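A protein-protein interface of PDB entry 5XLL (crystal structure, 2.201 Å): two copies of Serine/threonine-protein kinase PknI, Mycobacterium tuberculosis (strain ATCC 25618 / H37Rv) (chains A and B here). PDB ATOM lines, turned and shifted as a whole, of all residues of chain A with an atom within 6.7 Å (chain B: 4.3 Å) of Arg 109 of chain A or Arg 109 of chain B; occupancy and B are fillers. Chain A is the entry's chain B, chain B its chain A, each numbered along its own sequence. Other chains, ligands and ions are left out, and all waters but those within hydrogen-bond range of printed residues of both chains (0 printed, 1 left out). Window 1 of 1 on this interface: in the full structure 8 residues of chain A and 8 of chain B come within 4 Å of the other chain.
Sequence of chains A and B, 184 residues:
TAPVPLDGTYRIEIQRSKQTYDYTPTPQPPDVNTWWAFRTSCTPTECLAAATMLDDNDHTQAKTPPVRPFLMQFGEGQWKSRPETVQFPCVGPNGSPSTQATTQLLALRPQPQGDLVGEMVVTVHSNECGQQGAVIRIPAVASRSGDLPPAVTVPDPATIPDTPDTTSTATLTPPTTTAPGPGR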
ATOM      1  N   PHE A  74      19.201 -12.149  35.136  1.00  0.00           N
ATOM      2  CA  PHE A  74      18.221 -11.648  34.199  1.00  0.00           C
ATOM      3  C   PHE A  74      18.704 -10.368  33.525  1.00  0.00           C
ATOM      4  O   PHE A  74      19.007  -9.372  34.194  1.00  0.00           O
ATOM      5  CB  PHE A  74      16.879 -11.383  34.875  1.00  0.00           C
ATOM      6  CG  PHE A  74      15.771 -11.092  33.897  1.00  0.00           C
ATOM      7  CD1 PHE A  74      15.514  -9.784  33.482  1.00  0.00           C
ATOM      8  CD2 PHE A  74      15.012 -12.129  33.361  1.00  0.00           C
ATOM      9  CE1 PHE A  74      14.503  -9.511  32.559  1.00  0.00           C
ATOM     10  CE2 PHE A  74      14.005 -11.869  32.430  1.00  0.00           C
ATOM     11  CZ  PHE A  74      13.744 -10.555  32.033  1.00  0.00           C
ATOM     12  N   GLY A  75      18.757 -10.400  32.198  1.00  0.00           N
ATOM     13  CA  GLY A  75      19.052  -9.209  31.426  1.00  0.00           C
ATOM     14  C   GLY A  75      18.579  -9.342  29.993  1.00  0.00           C
ATOM     15  O   GLY A  75      18.610 -10.447  29.420  1.00  0.00           O
ATOM     16  N   GLU A  76      18.141  -8.215  29.427  1.00  0.00           N
ATOM     17  CA  GLU A  76      17.744  -8.151  28.024  1.00  0.00           C
ATOM     18  C   GLU A  76      16.637  -9.150  27.734  1.00  0.00           C
ATOM     19  O   GLU A  76      16.736  -9.940  26.788  1.00  0.00           O
ATOM     20  CB  GLU A  76      18.954  -8.398  27.109  1.00  0.00           C
ATOM     21  CG  GLU A  76      19.806  -7.152  26.851  1.00  0.00           C
ATOM     22  CD  GLU A  76      20.451  -6.589  28.110  1.00  0.00           C
ATOM     23  OE1 GLU A  76      21.437  -7.203  28.580  1.00  0.00           O
ATOM     24  OE2 GLU A  76      19.983  -5.528  28.611  1.00  0.00           O
ATOM     25  N   GLY A  77      15.606  -9.126  28.581  1.00  0.00           N
ATOM     26  CA  GLY A  77      14.434  -9.962  28.415  1.00  0.00           C
ATOM     27  C   GLY A  77      14.579 -11.453  28.706  1.00  0.00           C
ATOM     28  O   GLY A  77      13.653 -12.208  28.413  1.00  0.00           O
ATOM     29  N   GLN A  78      15.698 -11.900  29.277  1.00  0.00           N
ATOM     30  CA  GLN A  78      15.805 -13.332  29.592  1.00  0.00           C
ATOM     31  C   GLN A  78      16.643 -13.688  30.827  1.00  0.00           C
ATOM     32  O   GLN A  78      17.524 -12.921  31.253  1.00  0.00           O
ATOM     33  CB  GLN A  78      16.342 -14.118  28.384  1.00  0.00           C
ATOM     34  CG  GLN A  78      17.832 -13.915  28.148  1.00  0.00           C
ATOM     35  CD  GLN A  78      18.335 -14.678  26.943  1.00  0.00           C
ATOM     36  OE1 GLN A  78      17.561 -15.363  26.266  1.00  0.00           O
ATOM     37  NE2 GLN A  78      19.632 -14.559  26.657  1.00  0.00           N
ATOM     38  N   TRP A  79      16.361 -14.861  31.397  1.00  0.00           N
ATOM     39  CA  TRP A  79      17.247 -15.439  32.400  1.00  0.00           C
ATOM     40  C   TRP A  79      18.342 -16.201  31.684  1.00  0.00           C
ATOM     41  O   TRP A  79      18.055 -17.029  30.819  1.00  0.00           O
ATOM     42  CB  TRP A  79      16.488 -16.401  33.311  1.00  0.00           C
ATOM     43  CG  TRP A  79      15.498 -15.721  34.210  1.00  0.00           C
ATOM     44  CD1 TRP A  79      14.138 -15.676  34.061  1.00  0.00           C
ATOM     45  CD2 TRP A  79      15.798 -15.000  35.419  1.00  0.00           C
ATOM     46  NE1 TRP A  79      13.571 -14.977  35.111  1.00  0.00           N
ATOM     47  CE2 TRP A  79      14.571 -14.542  35.949  1.00  0.00           C
ATOM     48  CE3 TRP A  79      16.991 -14.701  36.103  1.00  0.00           C
ATOM     49  CZ2 TRP A  79      14.500 -13.795  37.136  1.00  0.00           C
ATOM     50  CZ3 TRP A  79      16.921 -13.960  37.271  1.00  0.00           C
ATOM     51  CH2 TRP A  79      15.681 -13.519  37.779  1.00  0.00           C
ATOM     52  N   ALA A 107      19.590 -20.586  28.711  1.00  0.00           N
ATOM     53  CA  ALA A 107      18.867 -19.325  28.599  1.00  0.00           C
ATOM     54  C   ALA A 107      17.374 -19.610  28.767  1.00  0.00           C
ATOM     55  O   ALA A 107      16.857 -20.577  28.210  1.00  0.00           O
ATOM     56  CB  ALA A 107      19.155 -18.660  27.254  1.00  0.00           C
ATOM     57  N   LEU A 108      16.681 -18.774  29.528  1.00  0.00           N
ATOM     58  CA  LEU A 108      15.280 -19.026  29.844  1.00  0.00           C
ATOM     59  C   LEU A 108      14.413 -17.757  29.730  1.00  0.00           C
ATOM     60  O   LEU A 108      14.605 -16.795  30.472  1.00  0.00           O
ATOM     61  CB  LEU A 108      15.173 -19.632  31.246  1.00  0.00           C
ATOM     62  CG  LEU A 108      14.698 -21.082  31.456  1.00  0.00           C
ATOM     63  CD1 LEU A 108      15.146 -22.058  30.388  1.00  0.00           C
ATOM     64  CD2 LEU A 108      15.128 -21.571  32.841  1.00  0.00           C
ATOM     65  N   ARG A 109      13.437 -17.778  28.828  1.00  0.00           N
ATOM     66  CA  ARG A 109      12.579 -16.618  28.598  1.00  0.00           C
ATOM     67  C   ARG A 109      11.193 -16.764  29.238  1.00  0.00           C
ATOM     68  O   ARG A 109      10.461 -17.720  28.959  1.00  0.00           O
ATOM     69  CB  ARG A 109      12.508 -16.342  27.098  1.00  0.00           C
ATOM     70  CG  ARG A 109      13.911 -16.294  26.529  1.00  0.00           C
ATOM     71  CD  ARG A 109      13.954 -16.412  25.069  1.00  0.00           C
ATOM     72  NE  ARG A 109      14.491 -17.691  24.621  1.00  0.00           N
ATOM     73  CZ  ARG A 109      15.766 -17.919  24.323  1.00  0.00           C
ATOM     74  NH1 ARG A 109      16.681 -16.963  24.463  1.00  0.00           N
ATOM     75  NH2 ARG A 109      16.126 -19.125  23.890  1.00  0.00           N
ATOM     76  N   PRO A 110      10.839 -15.816  30.118  1.00  0.00           N
ATOM     77  CA  PRO A 110       9.623 -15.950  30.931  1.00  0.00           C
ATOM     78  C   PRO A 110       8.354 -15.779  30.091  1.00  0.00           C
ATOM     79  O   PRO A 110       8.356 -15.002  29.124  1.00  0.00           O
ATOM     80  CB  PRO A 110       9.761 -14.822  31.964  1.00  0.00           C
ATOM     81  CG  PRO A 110      10.633 -13.791  31.296  1.00  0.00           C
ATOM     82  CD  PRO A 110      11.566 -14.554  30.382  1.00  0.00           C
ATOM     83  N   GLN A 111       7.306 -16.516  30.462  1.00  0.00           N
ATOM     84  CA  GLN A 111       6.020 -16.529  29.762  1.00  0.00           C
ATOM     85  C   GLN A 111       4.880 -16.214  30.739  1.00  0.00           C
ATOM     86  O   GLN A 111       4.989 -16.522  31.929  1.00  0.00           O
ATOM     87  CB  GLN A 111       5.791 -17.915  29.134  1.00  0.00           C
ATOM     88  CG  GLN A 111       5.624 -17.931  27.610  1.00  0.00           C
ATOM     89  CD  GLN A 111       6.918 -17.638  26.861  1.00  0.00           C
ATOM     90  OE1 GLN A 111       7.792 -16.919  27.354  1.00  0.00           O
ATOM     91  NE2 GLN A 111       7.043 -18.193  25.655  1.00  0.00           N
ATOM     92  N   ASP A 115       5.285 -19.767  33.214  1.00  0.00           N
ATOM     93  CA  ASP A 115       6.329 -20.717  32.845  1.00  0.00           C
ATOM     94  C   ASP A 115       7.486 -20.046  32.090  1.00  0.00           C
ATOM     95  O   ASP A 115       7.453 -18.837  31.835  1.00  0.00           O
ATOM     96  CB  ASP A 115       5.747 -21.881  32.035  1.00  0.00           C
ATOM     97  CG  ASP A 115       5.080 -22.918  32.914  1.00  0.00           C
ATOM     98  OD1 ASP A 115       5.170 -22.799  34.165  1.00  0.00           O
ATOM     99  OD2 ASP A 115       4.475 -23.861  32.350  1.00  0.00           O
ATOM    100  N   LEU A 116       8.517 -20.827  31.767  1.00  0.00           N
ATOM    101  CA  LEU A 116       9.661 -20.310  31.029  1.00  0.00           C
ATOM    102  C   LEU A 116      10.019 -21.244  29.884  1.00  0.00           C
ATOM    103  O   LEU A 116       9.752 -22.447  29.944  1.00  0.00           O
ATOM    104  CB  LEU A 116      10.874 -20.080  31.944  1.00  0.00           C
ATOM    105  CG  LEU A 116      10.653 -19.146  33.140  1.00  0.00           C
ATOM    106  CD1 LEU A 116      10.451 -19.947  34.446  1.00  0.00           C
ATOM    107  CD2 LEU A 116      11.793 -18.124  33.272  1.00  0.00           C
ATOM    108  N   VAL A 117      10.602 -20.683  28.829  1.00  0.00           N
ATOM    109  CA  VAL A 117      10.941 -21.443  27.641  1.00  0.00           C
ATOM    110  C   VAL A 117      12.240 -20.861  27.122  1.00  0.00           C
ATOM    111  O   VAL A 117      12.431 -19.656  27.178  1.00  0.00           O
ATOM    112  CB  VAL A 117       9.840 -21.318  26.543  1.00  0.00           C
ATOM    113  CG1 VAL A 117      10.306 -21.952  25.223  1.00  0.00           C
ATOM    114  CG2 VAL A 117       8.529 -21.958  27.011  1.00  0.00           C
ATOM    115  N   GLY A 118      13.140 -21.721  26.650  1.00  0.00           N
ATOM    116  CA  GLY A 118      14.396 -21.277  26.081  1.00  0.00           C
ATOM    117  C   GLY A 118      15.210 -22.458  25.608  1.00  0.00           C
ATOM    118  O   GLY A 118      14.667 -23.391  24.999  1.00  0.00           O
ATOM    119  N   GLU A 119      16.514 -22.435  25.880  1.00  0.00           N
ATOM    120  CA  GLU A 119      17.390 -23.497  25.394  1.00  0.00           C
ATOM    121  C   GLU A 119      18.711 -23.582  26.148  1.00  0.00           C
ATOM    122  O   GLU A 119      19.175 -22.624  26.782  1.00  0.00           O
ATOM    123  CB  GLU A 119      17.696 -23.298  23.893  1.00  0.00           C
ATOM    124  CG  GLU A 119      18.368 -21.951  23.631  1.00  0.00           C
ATOM    125  CD  GLU A 119      18.518 -21.591  22.149  1.00  0.00           C
ATOM    126  OE1 GLU A 119      17.882 -22.235  21.276  1.00  0.00           O
ATOM    127  OE2 GLU A 119      19.279 -20.642  21.859  1.00  0.00           O
ATOM    128  N   VAL A 121      22.666 -24.012  25.374  1.00  0.00           N
ATOM    129  CA  VAL A 121      23.561 -23.771  24.241  1.00  0.00           C
ATOM    130  C   VAL A 121      24.955 -24.331  24.521  1.00  0.00           C
ATOM    131  O   VAL A 121      25.642 -23.902  25.462  1.00  0.00           O
ATOM    132  CB  VAL A 121      23.647 -22.275  23.928  1.00  0.00           C
ATOM    133  CG1 VAL A 121      24.378 -22.041  22.616  1.00  0.00           C
ATOM    134  CG2 VAL A 121      22.245 -21.671  23.871  1.00  0.00           C
ATOM    135  N   GLU B  76      11.665 -21.050  20.763  1.00  0.00           N
ATOM    136  CA  GLU B  76      12.177 -21.151  22.126  1.00  0.00           C
ATOM    137  C   GLU B  76      12.061 -19.804  22.828  1.00  0.00           C
ATOM    138  O   GLU B  76      13.045 -19.292  23.378  1.00  0.00           O
ATOM    139  CB  GLU B  76      13.635 -21.641  22.124  1.00  0.00           C
ATOM    140  CG  GLU B  76      13.797 -23.151  21.930  1.00  0.00           C
ATOM    141  CD  GLU B  76      13.475 -23.619  20.521  1.00  0.00           C
ATOM    142  OE1 GLU B  76      14.115 -23.111  19.564  1.00  0.00           O
ATOM    143  OE2 GLU B  76      12.586 -24.503  20.372  1.00  0.00           O
ATOM    144  N   GLY B  77      10.862 -19.222  22.765  1.00  0.00           N
ATOM    145  CA  GLY B  77      10.556 -17.978  23.447  1.00  0.00           C
ATOM    146  C   GLY B  77      11.110 -16.673  22.877  1.00  0.00           C
ATOM    147  O   GLY B  77      10.929 -15.630  23.506  1.00  0.00           O
ATOM    148  N   GLN B  78      11.769 -16.691  21.717  1.00  0.00           N
ATOM    149  CA  GLN B  78      12.300 -15.421  21.178  1.00  0.00           C
ATOM    150  C   GLN B  78      12.277 -15.300  19.653  1.00  0.00           C
ATOM    151  O   GLN B  78      12.226 -16.315  18.938  1.00  0.00           O
ATOM    152  CB  GLN B  78      13.739 -15.176  21.668  1.00  0.00           C
ATOM    153  CG  GLN B  78      14.757 -16.113  21.034  1.00  0.00           C
ATOM    154  CD  GLN B  78      16.167 -15.887  21.552  1.00  0.00           C
ATOM    155  OE1 GLN B  78      16.394 -15.033  22.412  1.00  0.00           O
ATOM    156  NE2 GLN B  78      17.125 -16.659  21.036  1.00  0.00           N
ATOM    157  N   ALA B 107      18.710 -11.001  18.503  1.00  0.00           N
ATOM    158  CA  ALA B 107      17.669 -11.762  19.192  1.00  0.00           C
ATOM    159  C   ALA B 107      16.723 -10.778  19.894  1.00  0.00           C
ATOM    160  O   ALA B 107      17.165  -9.779  20.454  1.00  0.00           O
ATOM    161  CB  ALA B 107      18.288 -12.757  20.188  1.00  0.00           C
ATOM    162  N   LEU B 108      15.424 -11.054  19.859  1.00  0.00           N
ATOM    163  CA  LEU B 108      14.440 -10.115  20.386  1.00  0.00           C
ATOM    164  C   LEU B 108      13.333 -10.828  21.190  1.00  0.00           C
ATOM    165  O   LEU B 108      12.600 -11.661  20.659  1.00  0.00           O
ATOM    166  CB  LEU B 108      13.833  -9.322  19.229  1.00  0.00           C
ATOM    167  CG  LEU B 108      14.028  -7.805  19.095  1.00  0.00           C
ATOM    168  CD1 LEU B 108      15.431  -7.328  19.394  1.00  0.00           C
ATOM    169  CD2 LEU B 108      13.609  -7.374  17.685  1.00  0.00           C
ATOM    170  N   ARG B 109      13.193 -10.481  22.463  1.00  0.00           N
ATOM    171  CA  ARG B 109      12.228 -11.159  23.315  1.00  0.00           C
ATOM    172  C   ARG B 109      11.006 -10.296  23.630  1.00  0.00           C
ATOM    173  O   ARG B 109      11.126  -9.199  24.177  1.00  0.00           O
ATOM    174  CB  ARG B 109      12.933 -11.660  24.576  1.00  0.00           C
ATOM    175  CG  ARG B 109      14.102 -12.523  24.199  1.00  0.00           C
ATOM    176  CD  ARG B 109      15.070 -12.684  25.291  1.00  0.00           C
ATOM    177  NE  ARG B 109      16.267 -11.878  25.107  1.00  0.00           N
ATOM    178  CZ  ARG B 109      17.397 -12.314  24.556  1.00  0.00           C
ATOM    179  NH1 ARG B 109      17.486 -13.550  24.082  1.00  0.00           N
ATOM    180  NH2 ARG B 109      18.447 -11.499  24.476  1.00  0.00           N
ATOM    181  N   PRO B 110       9.816 -10.791  23.269  1.00  0.00           N
ATOM    182  CA  PRO B 110       8.608  -9.957  23.382  1.00  0.00           C
ATOM    183  C   PRO B 110       8.226  -9.606  24.831  1.00  0.00           C
ATOM    184  O   PRO B 110       8.576 -10.345  25.758  1.00  0.00           O
ATOM    185  CB  PRO B 110       7.518 -10.808  22.702  1.00  0.00           C
ATOM    186  CG  PRO B 110       8.040 -12.233  22.740  1.00  0.00           C
ATOM    187  CD  PRO B 110       9.545 -12.132  22.705  1.00  0.00           C
ATOM    188  N   GLN B 111       7.551  -8.466  24.995  1.00  0.00           N
ATOM    189  CA  GLN B 111       7.008  -8.006  26.277  1.00  0.00           C
ATOM    190  C   GLN B 111       5.527  -7.625  26.122  1.00  0.00           C
ATOM    191  O   GLN B 111       5.115  -7.180  25.047  1.00  0.00           O
ATOM    192  CB  GLN B 111       7.794  -6.788  26.804  1.00  0.00           C
ATOM    193  CG  GLN B 111       9.324  -6.871  26.689  1.00  0.00           C
ATOM    194  CD  GLN B 111       9.931  -8.024  27.486  1.00  0.00           C
ATOM    195  OE1 GLN B 111       9.235  -8.720  28.226  1.00  0.00           O
ATOM    196  NE2 GLN B 111      11.243  -8.226  27.341  1.00  0.00           N
ATOM    197  N   LEU B 116       9.707  -5.116  22.399  1.00  0.00           N
ATOM    198  CA  LEU B 116      10.620  -6.242  22.434  1.00  0.00           C
ATOM    199  C   LEU B 116      11.957  -5.789  23.004  1.00  0.00           C
ATOM    200  O   LEU B 116      12.338  -4.625  22.870  1.00  0.00           O
ATOM    201  CB  LEU B 116      10.792  -6.871  21.043  1.00  0.00           C
ATOM    202  CG  LEU B 116       9.515  -7.410  20.374  1.00  0.00           C
ATOM    203  CD1 LEU B 116       8.967  -6.436  19.326  1.00  0.00           C
ATOM    204  CD2 LEU B 116       9.734  -8.795  19.764  1.00  0.00           C
ATOM    205  N   VAL B 117      12.655  -6.702  23.674  1.00  0.00           N
ATOM    206  CA  VAL B 117      13.941  -6.394  24.268  1.00  0.00           C
ATOM    207  C   VAL B 117      14.803  -7.600  23.992  1.00  0.00           C
ATOM    208  O   VAL B 117      14.310  -8.717  24.000  1.00  0.00           O
ATOM    209  CB  VAL B 117      13.830  -6.175  25.797  1.00  0.00           C
ATOM    210  CG1 VAL B 117      15.214  -5.943  26.414  1.00  0.00           C
ATOM    211  CG2 VAL B 117      12.911  -4.995  26.101  1.00  0.00           C
ATOM    212  N   GLY B 118      16.080  -7.374  23.718  1.00  0.00           N
ATOM    213  CA  GLY B 118      17.004  -8.457  23.472  1.00  0.00           C
ATOM    214  C   GLY B 118      18.368  -7.880  23.204  1.00  0.00           C
ATOM    215  O   GLY B 118      18.790  -6.930  23.880  1.00  0.00           O
ATOM    216  N   GLU B 119      19.062  -8.436  22.211  1.00  0.00           N
ATOM    217  CA  GLU B 119      20.424  -8.007  21.919  1.00  0.00           C
ATOM    218  C   GLU B 119      20.908  -8.430  20.536  1.00  0.00           C
ATOM    219  O   GLU B 119      20.396  -9.363  19.911  1.00  0.00           O
ATOM    220  CB  GLU B 119      21.414  -8.539  22.988  1.00  0.00           C
ATOM    221  CG  GLU B 119      21.528 -10.065  22.985  1.00  0.00           C
ATOM    222  CD  GLU B 119      22.262 -10.643  24.202  1.00  0.00           C
ATOM    223  OE1 GLU B 119      22.594  -9.894  25.151  1.00  0.00           O
ATOM    224  OE2 GLU B 119      22.510 -11.867  24.212  1.00  0.00           O
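The backbone carbonyl oxygen (O) of Glu 76 of chain B sits at hydrogen-bond distance from the guanidinium group (NE) of Arg 109 of chain A, at 2.5 Å.
OE1 of Gln 78 of chain B sits at hydrogen-bond distance from NH1 of Arg 109 of chain A (2.8 Å).
NE of Arg 109 of chain B lies within hydrogen-bond range of O of Glu 76 of chain A (2.6 Å).
The guanidinium group (NH1) of Arg 109 of chain B is in hydrogen-bond range of the side-chain amide oxygen (OE1) of Gln 78 of chain A, 2.8 Å away.
The guanidinium group (NH1) of Arg 109 of chain B is in hydrogen-bond range of the side-chain amide oxygen (OE1) of Gln 78 of chain B, at 2.5 Å.
The backbone carbonyl oxygen of Arg 109 of chain B sits at hydrogen-bond distance from the side-chain amide nitrogen of Gln 111 of chain B (3.3 Å).
N of Arg 109 of chain B lies within hydrogen-bond range of O of Val 117 of chain B.
The side-chain amide oxygen of Gln 78 of chain A lies within hydrogen-bond range of the guanidinium group of Arg 109 of chain A.
The backbone carbonyl oxygen (O) of Arg 109 of chain A lies close to the side-chain amide oxygen (OE1) of Gln 111 of chain A.
O of Val 117 of chain A is in hydrogen-bond range of N of Arg 109 of chain A, 2.7 Å away.
Among the printed residues, pairs that only touch across the chains: Glu 76 of chain A with Gly 118 of chain B, Gly 118 of chain A with Glu 76 of chain B, Gly 77 of chain A with Arg 109 of chain B, Arg 109 of chain A with Gly 77 of chain B, Arg 109 of chain A with Arg 109 of chain B, Val 117 of chain A with Glu 76 of chain B, Val 117 of chain A with Gly 77 of chain B, Glu 76 of chain A with Val 117 of chain B, Gly 77 of chain A with Gln 111 of chain B and Gly 77 of chain A with Val 117 of chain B.
Arg 109 of chain A touches just these residues of chain B: Glu 76 (2.5 Å), Gly 77 (3.5 Å), Gln 78 (2.8 Å) and Arg 109 (3.5 Å).
Arg 109 of chain B touches just these residues of chain A: Glu 76, Gly 77, Gln 78 and Arg 109.
Printed residues of chain A within 4 Å of Gln 111 of chain B: Gly 77.
Of the printed residues of chain B, Val 117 of chain A touches Glu 76 and Gly 77.
Printed residues of chain B within 4 Å of Gly 118 of chain A: Glu 76.
Of the printed residues of chain A, Gln 78 of chain B touches Arg 109.
Gln 111 of chain A touches none of the printed residues of chain B.
The nearest printed residue of chain B that does not touch Arg 109 of chain A is Ala 107 of chain B (6.2 Å).
The nearest residue of chain A that does not touch Arg 109 of chain B is Gly 75 of chain A (5.1 Å).
Of the 12 printed residues of chain B, 7 touch a printed residue of chain A.
Printed residues of chain A that touch a printed residue of chain B: Glu 76, Gly 77, Gln 78, Arg 109, Val 117 and Gly 118.
Hydrophobic or aromatic side chains of chain A that line the printed part of chain B: Val 117.
Among the printed residues, 14 pairs touch across the chains.
Among the printed residues, no Asp or Glu carboxylate lies within 4 Å of a Lys or Arg side-chain nitrogen of the other chain.
Glu 76 of chain A touches Arg 109 of chain B, and with the chains exchanged Arg 109 of chain A touches Glu 76 of chain B.
Glu 76 of chain A touches Val 117 of chain B, and with the chains exchanged Val 117 of chain A touches Glu 76 of chain B.
Gly 77 of chain A touches Arg 109 of chain B, and with the chains exchanged Arg 109 of chain A touches Gly 77 of chain B.
Arg 109 of chain A touches its own counterpart, Arg 109 of chain B.
Positions printed for both chains: 76, 77, 78, 107, 108, 109, 110, 111, 116, 117, 118 and 119.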
